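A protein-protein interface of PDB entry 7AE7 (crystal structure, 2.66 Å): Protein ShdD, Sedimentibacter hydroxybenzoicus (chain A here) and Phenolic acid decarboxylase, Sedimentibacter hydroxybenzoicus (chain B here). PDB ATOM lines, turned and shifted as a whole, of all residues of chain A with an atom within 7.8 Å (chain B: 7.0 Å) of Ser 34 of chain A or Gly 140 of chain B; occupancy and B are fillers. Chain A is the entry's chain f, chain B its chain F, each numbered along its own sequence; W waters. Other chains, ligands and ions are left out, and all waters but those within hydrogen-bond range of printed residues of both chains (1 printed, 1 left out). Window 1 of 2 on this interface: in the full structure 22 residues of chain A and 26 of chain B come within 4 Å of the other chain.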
ATOM      1  N   CYS A   3     -20.202 -18.992  30.896  1.00  0.00           N
ATOM      2  CA  CYS A   3     -18.770 -19.123  31.126  1.00  0.00           C
ATOM      3  C   CYS A   3     -18.451 -20.489  31.725  1.00  0.00           C
ATOM      4  O   CYS A   3     -19.187 -20.999  32.575  1.00  0.00           O
ATOM      5  CB  CYS A   3     -18.287 -18.003  32.051  1.00  0.00           C
ATOM      6  SG  CYS A   3     -16.569 -18.124  32.604  1.00  0.00           S
ATOM      7  N   HIS A   4     -17.351 -21.089  31.269  1.00  0.00           N
ATOM      8  CA  HIS A   4     -16.954 -22.406  31.753  1.00  0.00           C
ATOM      9  C   HIS A   4     -16.225 -22.355  33.089  1.00  0.00           C
ATOM     10  O   HIS A   4     -16.044 -23.404  33.717  1.00  0.00           O
ATOM     11  CB  HIS A   4     -16.070 -23.103  30.716  1.00  0.00           C
ATOM     12  CG  HIS A   4     -16.819 -23.600  29.519  1.00  0.00           C
ATOM     13  ND1 HIS A   4     -17.510 -24.792  29.515  1.00  0.00           N
ATOM     14  CD2 HIS A   4     -16.991 -23.061  28.289  1.00  0.00           C
ATOM     15  CE1 HIS A   4     -18.071 -24.970  28.333  1.00  0.00           C
ATOM     16  NE2 HIS A   4     -17.772 -23.933  27.570  1.00  0.00           N
ATOM     17  N   ARG A   5     -15.811 -21.172  33.536  1.00  0.00           N
ATOM     18  CA  ARG A   5     -15.058 -21.029  34.774  1.00  0.00           C
ATOM     19  C   ARG A   5     -15.893 -20.478  35.922  1.00  0.00           C
ATOM     20  O   ARG A   5     -15.806 -20.988  37.043  1.00  0.00           O
ATOM     21  CB  ARG A   5     -13.842 -20.124  34.546  1.00  0.00           C
ATOM     22  CG  ARG A   5     -12.921 -20.008  35.746  1.00  0.00           C
ATOM     23  CD  ARG A   5     -11.521 -19.592  35.325  1.00  0.00           C
ATOM     24  NE  ARG A   5     -11.452 -18.178  34.974  1.00  0.00           N
ATOM     25  CZ  ARG A   5     -10.325 -17.492  34.846  1.00  0.00           C
ATOM     26  NH1 ARG A   5      -9.144 -18.060  35.031  1.00  0.00           N
ATOM     27  NH2 ARG A   5     -10.383 -16.203  34.524  1.00  0.00           N
ATOM     28  N   ARG A  12     -19.221 -12.543  25.940  1.00  0.00           N
ATOM     29  CA  ARG A  12     -19.135 -11.725  24.742  1.00  0.00           C
ATOM     30  C   ARG A  12     -18.184 -12.384  23.756  1.00  0.00           C
ATOM     31  O   ARG A  12     -17.118 -12.874  24.144  1.00  0.00           O
ATOM     32  CB  ARG A  12     -18.653 -10.305  25.080  1.00  0.00           C
ATOM     33  CG  ARG A  12     -18.019  -9.553  23.913  1.00  0.00           C
ATOM     34  CD  ARG A  12     -17.351  -8.256  24.365  1.00  0.00           C
ATOM     35  NE  ARG A  12     -16.035  -8.486  24.952  1.00  0.00           N
ATOM     36  CZ  ARG A  12     -15.057  -7.590  24.981  1.00  0.00           C
ATOM     37  NH1 ARG A  12     -15.205  -6.384  24.457  1.00  0.00           N
ATOM     38  NH2 ARG A  12     -13.900  -7.913  25.554  1.00  0.00           N
ATOM     39  N   MET A  14     -15.290 -12.446  21.393  1.00  0.00           N
ATOM     40  CA  MET A  14     -14.124 -11.582  21.264  1.00  0.00           C
ATOM     41  C   MET A  14     -13.826 -11.272  19.802  1.00  0.00           C
ATOM     42  O   MET A  14     -13.917 -10.117  19.371  1.00  0.00           O
ATOM     43  CB  MET A  14     -12.913 -12.234  21.936  1.00  0.00           C
ATOM     44  CG  MET A  14     -12.048 -11.264  22.713  1.00  0.00           C
ATOM     45  SD  MET A  14     -10.335 -11.804  22.814  1.00  0.00           S
ATOM     46  CE  MET A  14     -10.448 -13.027  24.114  1.00  0.00           C
ATOM     47  N   VAL A  25     -13.843 -16.793  19.128  1.00  0.00           N
ATOM     48  CA  VAL A  25     -13.278 -16.722  20.473  1.00  0.00           C
ATOM     49  C   VAL A  25     -14.284 -16.024  21.376  1.00  0.00           C
ATOM     50  O   VAL A  25     -14.715 -14.899  21.090  1.00  0.00           O
ATOM     51  CB  VAL A  25     -11.922 -16.001  20.488  1.00  0.00           C
ATOM     52  CG1 VAL A  25     -11.441 -15.825  21.919  1.00  0.00           C
ATOM     53  CG2 VAL A  25     -10.900 -16.781  19.679  1.00  0.00           C
ATOM     54  N   TYR A  26     -14.655 -16.689  22.466  1.00  0.00           N
ATOM     55  CA  TYR A  26     -15.600 -16.166  23.437  1.00  0.00           C
ATOM     56  C   TYR A  26     -14.865 -15.790  24.715  1.00  0.00           C
ATOM     57  O   TYR A  26     -13.890 -16.441  25.104  1.00  0.00           O
ATOM     58  CB  TYR A  26     -16.696 -17.189  23.743  1.00  0.00           C
ATOM     59  CG  TYR A  26     -17.470 -17.604  22.517  1.00  0.00           C
ATOM     60  CD1 TYR A  26     -18.369 -16.734  21.916  1.00  0.00           C
ATOM     61  CD2 TYR A  26     -17.288 -18.857  21.948  1.00  0.00           C
ATOM     62  CE1 TYR A  26     -19.074 -17.102  20.789  1.00  0.00           C
ATOM     63  CE2 TYR A  26     -17.989 -19.236  20.821  1.00  0.00           C
ATOM     64  CZ  TYR A  26     -18.880 -18.354  20.246  1.00  0.00           C
ATOM     65  OH  TYR A  26     -19.581 -18.723  19.122  1.00  0.00           O
ATOM     66  N   VAL A  27     -15.332 -14.723  25.356  1.00  0.00           N
ATOM     67  CA  VAL A  27     -14.719 -14.218  26.577  1.00  0.00           C
ATOM     68  C   VAL A  27     -15.821 -13.836  27.557  1.00  0.00           C
ATOM     69  O   VAL A  27     -16.868 -13.310  27.164  1.00  0.00           O
ATOM     70  CB  VAL A  27     -13.779 -13.025  26.291  1.00  0.00           C
ATOM     71  CG1 VAL A  27     -14.539 -11.864  25.667  1.00  0.00           C
ATOM     72  CG2 VAL A  27     -13.063 -12.588  27.561  1.00  0.00           C
ATOM     73  N   CYS A  28     -15.591 -14.131  28.831  1.00  0.00           N
ATOM     74  CA  CYS A  28     -16.511 -13.761  29.896  1.00  0.00           C
ATOM     75  C   CYS A  28     -16.111 -12.407  30.467  1.00  0.00           C
ATOM     76  O   CYS A  28     -14.950 -12.200  30.835  1.00  0.00           O
ATOM     77  CB  CYS A  28     -16.513 -14.829  30.990  1.00  0.00           C
ATOM     78  SG  CYS A  28     -16.884 -14.216  32.641  1.00  0.00           S
ATOM     79  N   CYS A  31     -14.986 -12.636  34.631  1.00  0.00           N
ATOM     80  CA  CYS A  31     -13.767 -13.233  35.160  1.00  0.00           C
ATOM     81  C   CYS A  31     -12.631 -13.340  34.150  1.00  0.00           C
ATOM     82  O   CYS A  31     -11.593 -13.927  34.477  1.00  0.00           O
ATOM     83  CB  CYS A  31     -14.070 -14.627  35.732  1.00  0.00           C
ATOM     84  SG  CYS A  31     -14.041 -15.957  34.512  1.00  0.00           S
ATOM     85  N   CYS A  32     -12.800 -12.808  32.938  1.00  0.00           N
ATOM     86  CA  CYS A  32     -11.790 -12.688  31.888  1.00  0.00           C
ATOM     87  C   CYS A  32     -11.454 -14.006  31.199  1.00  0.00           C
ATOM     88  O   CYS A  32     -10.591 -14.015  30.315  1.00  0.00           O
ATOM     89  CB  CYS A  32     -10.480 -12.063  32.395  1.00  0.00           C
ATOM     90  SG  CYS A  32     -10.578 -10.299  32.776  1.00  0.00           S
ATOM     91  N   TYR A  33     -12.092 -15.117  31.570  1.00  0.00           N
ATOM     92  CA  TYR A  33     -11.829 -16.381  30.895  1.00  0.00           C
ATOM     93  C   TYR A  33     -12.198 -16.283  29.419  1.00  0.00           C
ATOM     94  O   TYR A  33     -13.218 -15.695  29.053  1.00  0.00           O
ATOM     95  CB  TYR A  33     -12.616 -17.515  31.554  1.00  0.00           C
ATOM     96  CG  TYR A  33     -12.196 -18.899  31.103  1.00  0.00           C
ATOM     97  CD1 TYR A  33     -10.989 -19.451  31.518  1.00  0.00           C
ATOM     98  CD2 TYR A  33     -13.007 -19.655  30.264  1.00  0.00           C
ATOM     99  CE1 TYR A  33     -10.601 -20.715  31.110  1.00  0.00           C
ATOM    100  CE2 TYR A  33     -12.628 -20.921  29.851  1.00  0.00           C
ATOM    101  CZ  TYR A  33     -11.424 -21.445  30.276  1.00  0.00           C
ATOM    102  OH  TYR A  33     -11.046 -22.703  29.866  1.00  0.00           O
ATOM    103  N   SER A  34     -11.352 -16.863  28.570  1.00  0.00           N
ATOM    104  CA  SER A  34     -11.597 -16.915  27.136  1.00  0.00           C
ATOM    105  C   SER A  34     -11.384 -18.337  26.639  1.00  0.00           C
ATOM    106  O   SER A  34     -10.612 -19.106  27.218  1.00  0.00           O
ATOM    107  CB  SER A  34     -10.682 -15.951  26.364  1.00  0.00           C
ATOM    108  OG  SER A  34      -9.407 -15.852  26.974  1.00  0.00           O
ATOM    109  N   TRP A  35     -12.083 -18.679  25.560  1.00  0.00           N
ATOM    110  CA  TRP A  35     -11.943 -20.001  24.968  1.00  0.00           C
ATOM    111  C   TRP A  35     -12.376 -19.955  23.510  1.00  0.00           C
ATOM    112  O   TRP A  35     -13.070 -19.033  23.075  1.00  0.00           O
ATOM    113  CB  TRP A  35     -12.746 -21.053  25.743  1.00  0.00           C
ATOM    114  CG  TRP A  35     -14.225 -20.920  25.599  1.00  0.00           C
ATOM    115  CD1 TRP A  35     -15.033 -21.621  24.753  1.00  0.00           C
ATOM    116  CD2 TRP A  35     -15.082 -20.032  26.327  1.00  0.00           C
ATOM    117  NE1 TRP A  35     -16.339 -21.224  24.906  1.00  0.00           N
ATOM    118  CE2 TRP A  35     -16.396 -20.249  25.867  1.00  0.00           C
ATOM    119  CE3 TRP A  35     -14.865 -19.072  27.321  1.00  0.00           C
ATOM    120  CZ2 TRP A  35     -17.489 -19.542  26.367  1.00  0.00           C
ATOM    121  CZ3 TRP A  35     -15.952 -18.371  27.816  1.00  0.00           C
ATOM    122  CH2 TRP A  35     -17.246 -18.610  27.338  1.00  0.00           C
ATOM    123  N   ARG A  36     -11.951 -20.964  22.758  1.00  0.00           N
ATOM    124  CA  ARG A  36     -12.252 -21.038  21.338  1.00  0.00           C
ATOM    125  C   ARG A  36     -13.480 -21.903  21.089  1.00  0.00           C
ATOM    126  O   ARG A  36     -13.791 -22.818  21.856  1.00  0.00           O
ATOM    127  CB  ARG A  36     -11.063 -21.586  20.545  1.00  0.00           C
ATOM    128  CG  ARG A  36     -11.007 -21.059  19.117  1.00  0.00           C
ATOM    129  CD  ARG A  36      -9.894 -21.706  18.312  1.00  0.00           C
ATOM    130  NE  ARG A  36      -8.585 -21.468  18.906  1.00  0.00           N
ATOM    131  CZ  ARG A  36      -7.868 -20.368  18.719  1.00  0.00           C
ATOM    132  NH1 ARG A  36      -8.303 -19.381  17.955  1.00  0.00           N
ATOM    133  NH2 ARG A  36      -6.686 -20.256  19.316  1.00  0.00           N
ATOM    134  N   GLU A  39     -12.694 -25.719  20.799  1.00  0.00           N
ATOM    135  CA  GLU A  39     -12.236 -26.484  21.949  1.00  0.00           C
ATOM    136  C   GLU A  39     -13.374 -26.686  22.944  1.00  0.00           C
ATOM    137  O   GLU A  39     -14.292 -25.868  23.045  1.00  0.00           O
ATOM    138  CB  GLU A  39     -11.045 -25.810  22.638  1.00  0.00           C
ATOM    139  CG  GLU A  39     -11.330 -24.480  23.313  1.00  0.00           C
ATOM    140  CD  GLU A  39     -10.068 -23.841  23.875  1.00  0.00           C
ATOM    141  OE1 GLU A  39      -9.055 -24.557  24.026  1.00  0.00           O
ATOM    142  OE2 GLU A  39     -10.089 -22.627  24.164  1.00  0.00           O
ATOM    143  N   PRO A  41     -13.768 -26.812  26.624  1.00  0.00           N
ATOM    144  CA  PRO A  41     -13.063 -26.563  27.889  1.00  0.00           C
ATOM    145  C   PRO A  41     -13.835 -27.137  29.068  1.00  0.00           C
ATOM    146  O   PRO A  41     -15.000 -26.795  29.289  1.00  0.00           O
ATOM    147  CB  PRO A  41     -12.988 -25.031  27.957  1.00  0.00           C
ATOM    148  CG  PRO A  41     -14.051 -24.531  27.008  1.00  0.00           C
ATOM    149  CD  PRO A  41     -14.700 -25.715  26.321  1.00  0.00           C
ATOM    150  N   PHE B 126      -5.311 -10.911  17.064  1.00  0.00           N
ATOM    151  CA  PHE B 126      -5.524 -12.181  16.381  1.00  0.00           C
ATOM    152  C   PHE B 126      -5.290 -12.080  14.880  1.00  0.00           C
ATOM    153  O   PHE B 126      -5.025 -13.103  14.238  1.00  0.00           O
ATOM    154  CB  PHE B 126      -6.937 -12.694  16.661  1.00  0.00           C
ATOM    155  CG  PHE B 126      -7.186 -13.009  18.107  1.00  0.00           C
ATOM    156  CD1 PHE B 126      -7.482 -12.001  19.010  1.00  0.00           C
ATOM    157  CD2 PHE B 126      -7.118 -14.312  18.566  1.00  0.00           C
ATOM    158  CE1 PHE B 126      -7.708 -12.287  20.342  1.00  0.00           C
ATOM    159  CE2 PHE B 126      -7.343 -14.608  19.896  1.00  0.00           C
ATOM    160  CZ  PHE B 126      -7.639 -13.593  20.786  1.00  0.00           C
ATOM    161  N   TYR B 132      -2.993 -19.127  20.758  1.00  0.00           N
ATOM    162  CA  TYR B 132      -3.503 -20.443  21.112  1.00  0.00           C
ATOM    163  C   TYR B 132      -3.378 -20.610  22.618  1.00  0.00           C
ATOM    164  O   TYR B 132      -2.756 -19.794  23.303  1.00  0.00           O
ATOM    165  CB  TYR B 132      -2.747 -21.555  20.374  1.00  0.00           C
ATOM    166  CG  TYR B 132      -1.263 -21.576  20.666  1.00  0.00           C
ATOM    167  CD1 TYR B 132      -0.394 -20.705  20.021  1.00  0.00           C
ATOM    168  CD2 TYR B 132      -0.732 -22.462  21.595  1.00  0.00           C
ATOM    169  CE1 TYR B 132       0.959 -20.720  20.288  1.00  0.00           C
ATOM    170  CE2 TYR B 132       0.621 -22.484  21.868  1.00  0.00           C
ATOM    171  CZ  TYR B 132       1.460 -21.610  21.213  1.00  0.00           C
ATOM    172  OH  TYR B 132       2.810 -21.626  21.478  1.00  0.00           O
ATOM    173  N   ARG B 133      -3.975 -21.681  23.136  1.00  0.00           N
ATOM    174  CA  ARG B 133      -3.873 -21.983  24.556  1.00  0.00           C
ATOM    175  C   ARG B 133      -2.699 -22.922  24.796  1.00  0.00           C
ATOM    176  O   ARG B 133      -2.599 -23.981  24.168  1.00  0.00           O
ATOM    177  CB  ARG B 133      -5.165 -22.597  25.091  1.00  0.00           C
ATOM    178  CG  ARG B 133      -5.373 -22.325  26.571  1.00  0.00           C
ATOM    179  CD  ARG B 133      -6.379 -23.276  27.187  1.00  0.00           C
ATOM    180  NE  ARG B 133      -7.743 -22.990  26.760  1.00  0.00           N
ATOM    181  CZ  ARG B 133      -8.446 -21.931  27.142  1.00  0.00           C
ATOM    182  NH1 ARG B 133      -7.945 -21.027  27.968  1.00  0.00           N
ATOM    183  NH2 ARG B 133      -9.685 -21.780  26.687  1.00  0.00           N
ATOM    184  N   ILE B 134      -1.814 -22.525  25.709  1.00  0.00           N
ATOM    185  CA  ILE B 134      -0.566 -23.251  25.912  1.00  0.00           C
ATOM    186  C   ILE B 134      -0.777 -24.469  26.803  1.00  0.00           C
ATOM    187  O   ILE B 134      -0.228 -25.545  26.541  1.00  0.00           O
ATOM    188  CB  ILE B 134       0.499 -22.294  26.476  1.00  0.00           C
ATOM    189  CG1 ILE B 134       0.823 -21.214  25.439  1.00  0.00           C
ATOM    190  CG2 ILE B 134       1.751 -23.056  26.888  1.00  0.00           C
ATOM    191  CD1 ILE B 134       1.828 -20.190  25.906  1.00  0.00           C
ATOM    192  N   ASN B 135      -1.570 -24.332  27.861  1.00  0.00           N
ATOM    193  CA  ASN B 135      -1.858 -25.448  28.749  1.00  0.00           C
ATOM    194  C   ASN B 135      -3.353 -25.515  29.026  1.00  0.00           C
ATOM    195  O   ASN B 135      -4.064 -24.510  28.948  1.00  0.00           O
ATOM    196  CB  ASN B 135      -1.070 -25.347  30.059  1.00  0.00           C
ATOM    197  CG  ASN B 135       0.336 -25.905  29.933  1.00  0.00           C
ATOM    198  OD1 ASN B 135       0.524 -27.084  29.629  1.00  0.00           O
ATOM    199  ND2 ASN B 135       1.330 -25.057  30.162  1.00  0.00           N
ATOM    200  N   GLN B 137      -5.435 -25.716  31.434  1.00  0.00           N
ATOM    201  CA  GLN B 137      -6.143 -24.925  32.432  1.00  0.00           C
ATOM    202  C   GLN B 137      -5.720 -23.459  32.438  1.00  0.00           C
ATOM    203  O   GLN B 137      -5.981 -22.753  33.419  1.00  0.00           O
ATOM    204  CB  GLN B 137      -5.953 -25.532  33.822  1.00  0.00           C
ATOM    205  CG  GLN B 137      -6.515 -26.936  33.969  1.00  0.00           C
ATOM    206  CD  GLN B 137      -8.022 -26.979  33.805  1.00  0.00           C
ATOM    207  OE1 GLN B 137      -8.753 -26.264  34.492  1.00  0.00           O
ATOM    208  NE2 GLN B 137      -8.494 -27.819  32.889  1.00  0.00           N
ATOM    209  N   ASP B 138      -5.072 -22.987  31.377  1.00  0.00           N
ATOM    210  CA  ASP B 138      -4.714 -21.578  31.294  1.00  0.00           C
ATOM    211  C   ASP B 138      -5.967 -20.713  31.209  1.00  0.00           C
ATOM    212  O   ASP B 138      -6.993 -21.116  30.654  1.00  0.00           O
ATOM    213  CB  ASP B 138      -3.817 -21.322  30.081  1.00  0.00           C
ATOM    214  CG  ASP B 138      -2.380 -21.759  30.310  1.00  0.00           C
ATOM    215  OD1 ASP B 138      -2.038 -22.115  31.458  1.00  0.00           O
ATOM    216  OD2 ASP B 138      -1.590 -21.740  29.341  1.00  0.00           O
ATOM    217  N   GLY B 139      -5.877 -19.506  31.770  1.00  0.00           N
ATOM    218  CA  GLY B 139      -7.005 -18.591  31.751  1.00  0.00           C
ATOM    219  C   GLY B 139      -7.326 -18.018  30.387  1.00  0.00           C
ATOM    220  O   GLY B 139      -8.393 -17.417  30.222  1.00  0.00           O
ATOM    221  N   GLY B 140      -6.438 -18.191  29.419  1.00  0.00           N
ATOM    222  CA  GLY B 140      -6.681 -17.681  28.086  1.00  0.00           C
ATOM    223  C   GLY B 140      -5.485 -17.943  27.203  1.00  0.00           C
ATOM    224  O   GLY B 140      -4.648 -18.794  27.507  1.00  0.00           O
ATOM    225  N   PHE B 141      -5.410 -17.204  26.100  1.00  0.00           N
ATOM    226  CA  PHE B 141      -4.285 -17.306  25.183  1.00  0.00           C
ATOM    227  C   PHE B 141      -3.176 -16.375  25.656  1.00  0.00           C
ATOM    228  O   PHE B 141      -3.430 -15.206  25.963  1.00  0.00           O
ATOM    229  CB  PHE B 141      -4.710 -16.962  23.756  1.00  0.00           C
ATOM    230  CG  PHE B 141      -5.901 -17.744  23.269  1.00  0.00           C
ATOM    231  CD1 PHE B 141      -6.178 -19.007  23.771  1.00  0.00           C
ATOM    232  CD2 PHE B 141      -6.746 -17.213  22.310  1.00  0.00           C
ATOM    233  CE1 PHE B 141      -7.274 -19.723  23.326  1.00  0.00           C
ATOM    234  CE2 PHE B 141      -7.843 -17.925  21.860  1.00  0.00           C
ATOM    235  CZ  PHE B 141      -8.107 -19.182  22.368  1.00  0.00           C
ATOM    236  N   TYR B 142      -1.954 -16.894  25.721  1.00  0.00           N
ATOM    237  CA  TYR B 142      -0.842 -16.179  26.326  1.00  0.00           C
ATOM    238  C   TYR B 142       0.249 -15.885  25.308  1.00  0.00           C
ATOM    239  O   TYR B 142       0.453 -16.634  24.348  1.00  0.00           O
ATOM    240  CB  TYR B 142      -0.234 -16.975  27.486  1.00  0.00           C
ATOM    241  CG  TYR B 142      -0.867 -16.697  28.827  1.00  0.00           C
ATOM    242  CD1 TYR B 142      -2.083 -17.271  29.174  1.00  0.00           C
ATOM    243  CD2 TYR B 142      -0.246 -15.866  29.750  1.00  0.00           C
ATOM    244  CE1 TYR B 142      -2.663 -17.022  30.405  1.00  0.00           C
ATOM    245  CE2 TYR B 142      -0.817 -15.610  30.981  1.00  0.00           C
ATOM    246  CZ  TYR B 142      -2.026 -16.191  31.303  1.00  0.00           C
ATOM    247  OH  TYR B 142      -2.601 -15.939  32.527  1.00  0.00           O
ATOM    248  N   GLN B 170      -1.225 -12.166  28.980  1.00  0.00           N
ATOM    249  CA  GLN B 170      -2.490 -12.833  28.703  1.00  0.00           C
ATOM    250  C   GLN B 170      -3.370 -11.947  27.833  1.00  0.00           C
ATOM    251  O   GLN B 170      -3.650 -10.798  28.187  1.00  0.00           O
ATOM    252  CB  GLN B 170      -3.231 -13.175  29.996  1.00  0.00           C
ATOM    253  CG  GLN B 170      -4.629 -13.740  29.751  1.00  0.00           C
ATOM    254  CD  GLN B 170      -5.432 -13.925  31.027  1.00  0.00           C
ATOM    255  OE1 GLN B 170      -5.040 -13.459  32.095  1.00  0.00           O
ATOM    256  NE2 GLN B 170      -6.566 -14.610  30.918  1.00  0.00           N
ATOM    257  N   VAL B 171      -3.825 -12.495  26.709  1.00  0.00           N
ATOM    258  CA  VAL B 171      -4.685 -11.744  25.803  1.00  0.00           C
ATOM    259  C   VAL B 171      -6.077 -11.649  26.416  1.00  0.00           C
ATOM    260  O   VAL B 171      -6.731 -12.666  26.676  1.00  0.00           O
ATOM    261  CB  VAL B 171      -4.725 -12.400  24.418  1.00  0.00           C
ATOM    262  CG1 VAL B 171      -5.900 -11.870  23.613  1.00  0.00           C
ATOM    263  CG2 VAL B 171      -3.415 -12.158  23.685  1.00  0.00           C
ATOM    264  N   LYS B 172      -6.534 -10.419  26.652  1.00  0.00           N
ATOM    265  CA  LYS B 172      -7.849 -10.174  27.226  1.00  0.00           C
ATOM    266  C   LYS B 172      -8.873  -9.723  26.197  1.00  0.00           C
ATOM    267  O   LYS B 172     -10.076  -9.901  26.418  1.00  0.00           O
ATOM    268  CB  LYS B 172      -7.757  -9.114  28.330  1.00  0.00           C
ATOM    269  CG  LYS B 172      -6.647  -9.363  29.336  1.00  0.00           C
ATOM    270  CD  LYS B 172      -7.035 -10.445  30.325  1.00  0.00           C
ATOM    271  CE  LYS B 172      -6.449 -10.164  31.697  1.00  0.00           C
ATOM    272  NZ  LYS B 172      -7.512 -10.025  32.731  1.00  0.00           N
ATOM    273  N   GLY B 274      -4.703 -15.129  34.906  1.00  0.00           N
ATOM    274  CA  GLY B 274      -4.336 -16.478  35.249  1.00  0.00           C
ATOM    275  C   GLY B 274      -5.523 -17.418  35.226  1.00  0.00           C
ATOM    276  O   GLY B 274      -6.647 -17.029  34.895  1.00  0.00           O
ATOM    277  N   PRO B 275      -5.294 -18.690  35.582  1.00  0.00           N
ATOM    278  CA  PRO B 275      -3.977 -19.222  35.948  1.00  0.00           C
ATOM    279  C   PRO B 275      -3.066 -19.452  34.746  1.00  0.00           C
ATOM    280  O   PRO B 275      -3.527 -19.430  33.604  1.00  0.00           O
ATOM    281  CB  PRO B 275      -4.321 -20.549  36.626  1.00  0.00           C
ATOM    282  CG  PRO B 275      -5.584 -20.967  35.985  1.00  0.00           C
ATOM    283  CD  PRO B 275      -6.355 -19.697  35.756  1.00  0.00           C
ATOM    284  N   PHE B 276      -1.777 -19.655  35.010  1.00  0.00           N
ATOM    285  CA  PHE B 276      -0.809 -19.919  33.957  1.00  0.00           C
ATOM    286  C   PHE B 276       0.315 -20.768  34.528  1.00  0.00           C
ATOM    287  O   PHE B 276       0.552 -20.786  35.739  1.00  0.00           O
ATOM    288  CB  PHE B 276      -0.256 -18.620  33.358  1.00  0.00           C
ATOM    289  CG  PHE B 276       0.606 -18.830  32.146  1.00  0.00           C
ATOM    290  CD1 PHE B 276       0.048 -19.233  30.946  1.00  0.00           C
ATOM    291  CD2 PHE B 276       1.973 -18.622  32.206  1.00  0.00           C
ATOM    292  CE1 PHE B 276       0.838 -19.427  29.829  1.00  0.00           C
ATOM    293  CE2 PHE B 276       2.768 -18.814  31.093  1.00  0.00           C
ATOM    294  CZ  PHE B 276       2.199 -19.217  29.901  1.00  0.00           C
HETATM  295  O   HOH W   1      -7.118 -15.317  25.527  1.00  0.00           O
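O of Ser 34 of chain A sits at hydrogen-bond distance from NH2 of Arg 133 of chain B (2.9 Å).
NH2 of Arg 133 of chain B is in salt-bridge range of OE2 of Glu 39 of chain A.
O of Gly 139 of chain B sits at hydrogen-bond distance from N of Ser 34 of chain A, at 3.4 Å.
The side-chain sulfur (SG) of Cys 32 of chain A sits at hydrogen-bond distance from the side-chain amino group (NZ) of Lys 172 of chain B (3.1 Å).
The backbone carbonyl oxygen of Gly 274 of chain B lies within hydrogen-bond range of the guanidinium group of Arg 5 of chain A, 2.7 Å away.
The backbone carbonyl oxygen (O) of Asp 138 of chain B is in hydrogen-bond range of the guanidinium group (NH1) of Arg 133 of chain B.
The backbone carbonyl oxygen (O) of Pro 275 of chain B lies within hydrogen-bond range of the backbone NH (N) of Gly 139 of chain B, at 3.0 Å.
OH of Tyr 142 of chain B sits close to N of Gly 274 of chain B (3.3 Å).
N of Gly 274 of chain B sits at hydrogen-bond distance from OE1 of Gln 170 of chain B (3.3 Å).
N of Tyr 33 of chain A lies close to SG of Cys 31 of chain A, at 3.6 Å.
The backbone NH (N) of Arg 36 of chain A is in hydrogen-bond range of the side-chain carboxylate (OE2) of Glu 39 of chain A, at 2.9 Å.
Among the printed residues, pairs that only touch across the chains: Arg 5 of chain A with Gly 139 of chain B, Arg 5 of chain A with Pro 275 of chain B, Met 14 of chain A with Phe 126 of chain B, Met 14 of chain A with Lys 172 of chain B, Val 25 of chain A with Phe 141 of chain B, Tyr 33 of chain A with Arg 133 of chain B, Tyr 33 of chain A with Asp 138 of chain B, Tyr 33 of chain A with Gly 139 of chain B, Ser 34 of chain A with Gly 140 of chain B, Trp 35 of chain A with Arg 133 of chain B, Arg 36 of chain A with Tyr 132 of chain B and Arg 36 of chain A with Phe 141 of chain B.
Val 27 of chain A touches none of the printed residues of chain B.
Of chain B, only Arg 133, Gly 139 and Gly 140 come within 4 Å of Ser 34 of chain A.
Of the printed residues of chain B, Trp 35 of chain A touches Arg 133.
Asn 135 of chain B touches none of the printed residues of chain A.
Of chain A, only Arg 5, Tyr 33 and Ser 34 come within 4 Å of Gly 139 of chain B.
Of chain A, only Ser 34 comes within 4 Å of Gly 140 of chain B.
Of the printed residues of chain A, Pro 275 of chain B touches Arg 5.
The nearest residue of chain B that does not touch Ser 34 of chain A is Val 171 of chain B (4.2 Å).
The nearest printed residue of chain A that does not touch Arg 133 of chain B is Arg 36 of chain A (4.6 Å).
Of the 17 printed residues of chain B, 10 touch a printed residue of chain A.
Hydrophobic or aromatic side chains of chain B that line the printed part of chain A: Phe 126, Phe 141 and Pro 275.
Along chain B the printed residues that touch a printed residue of chain A span positions 126 to 275.
Among the printed residues, Asp or Glu carboxylates within 4 Å of a Lys or Arg side-chain nitrogen of the other chain: Glu 39 of chain A with Arg 133 of chain B.
Water W1 lies within hydrogen-bond range of the backbone NH (N) of Phe 141 of chain B (2.6 Å), the side-chain hydroxyl (OG) of Ser 34 of chain A (2.8 Å) and the backbone carbonyl oxygen (O) of Val 171 of chain B (2.9 Å).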
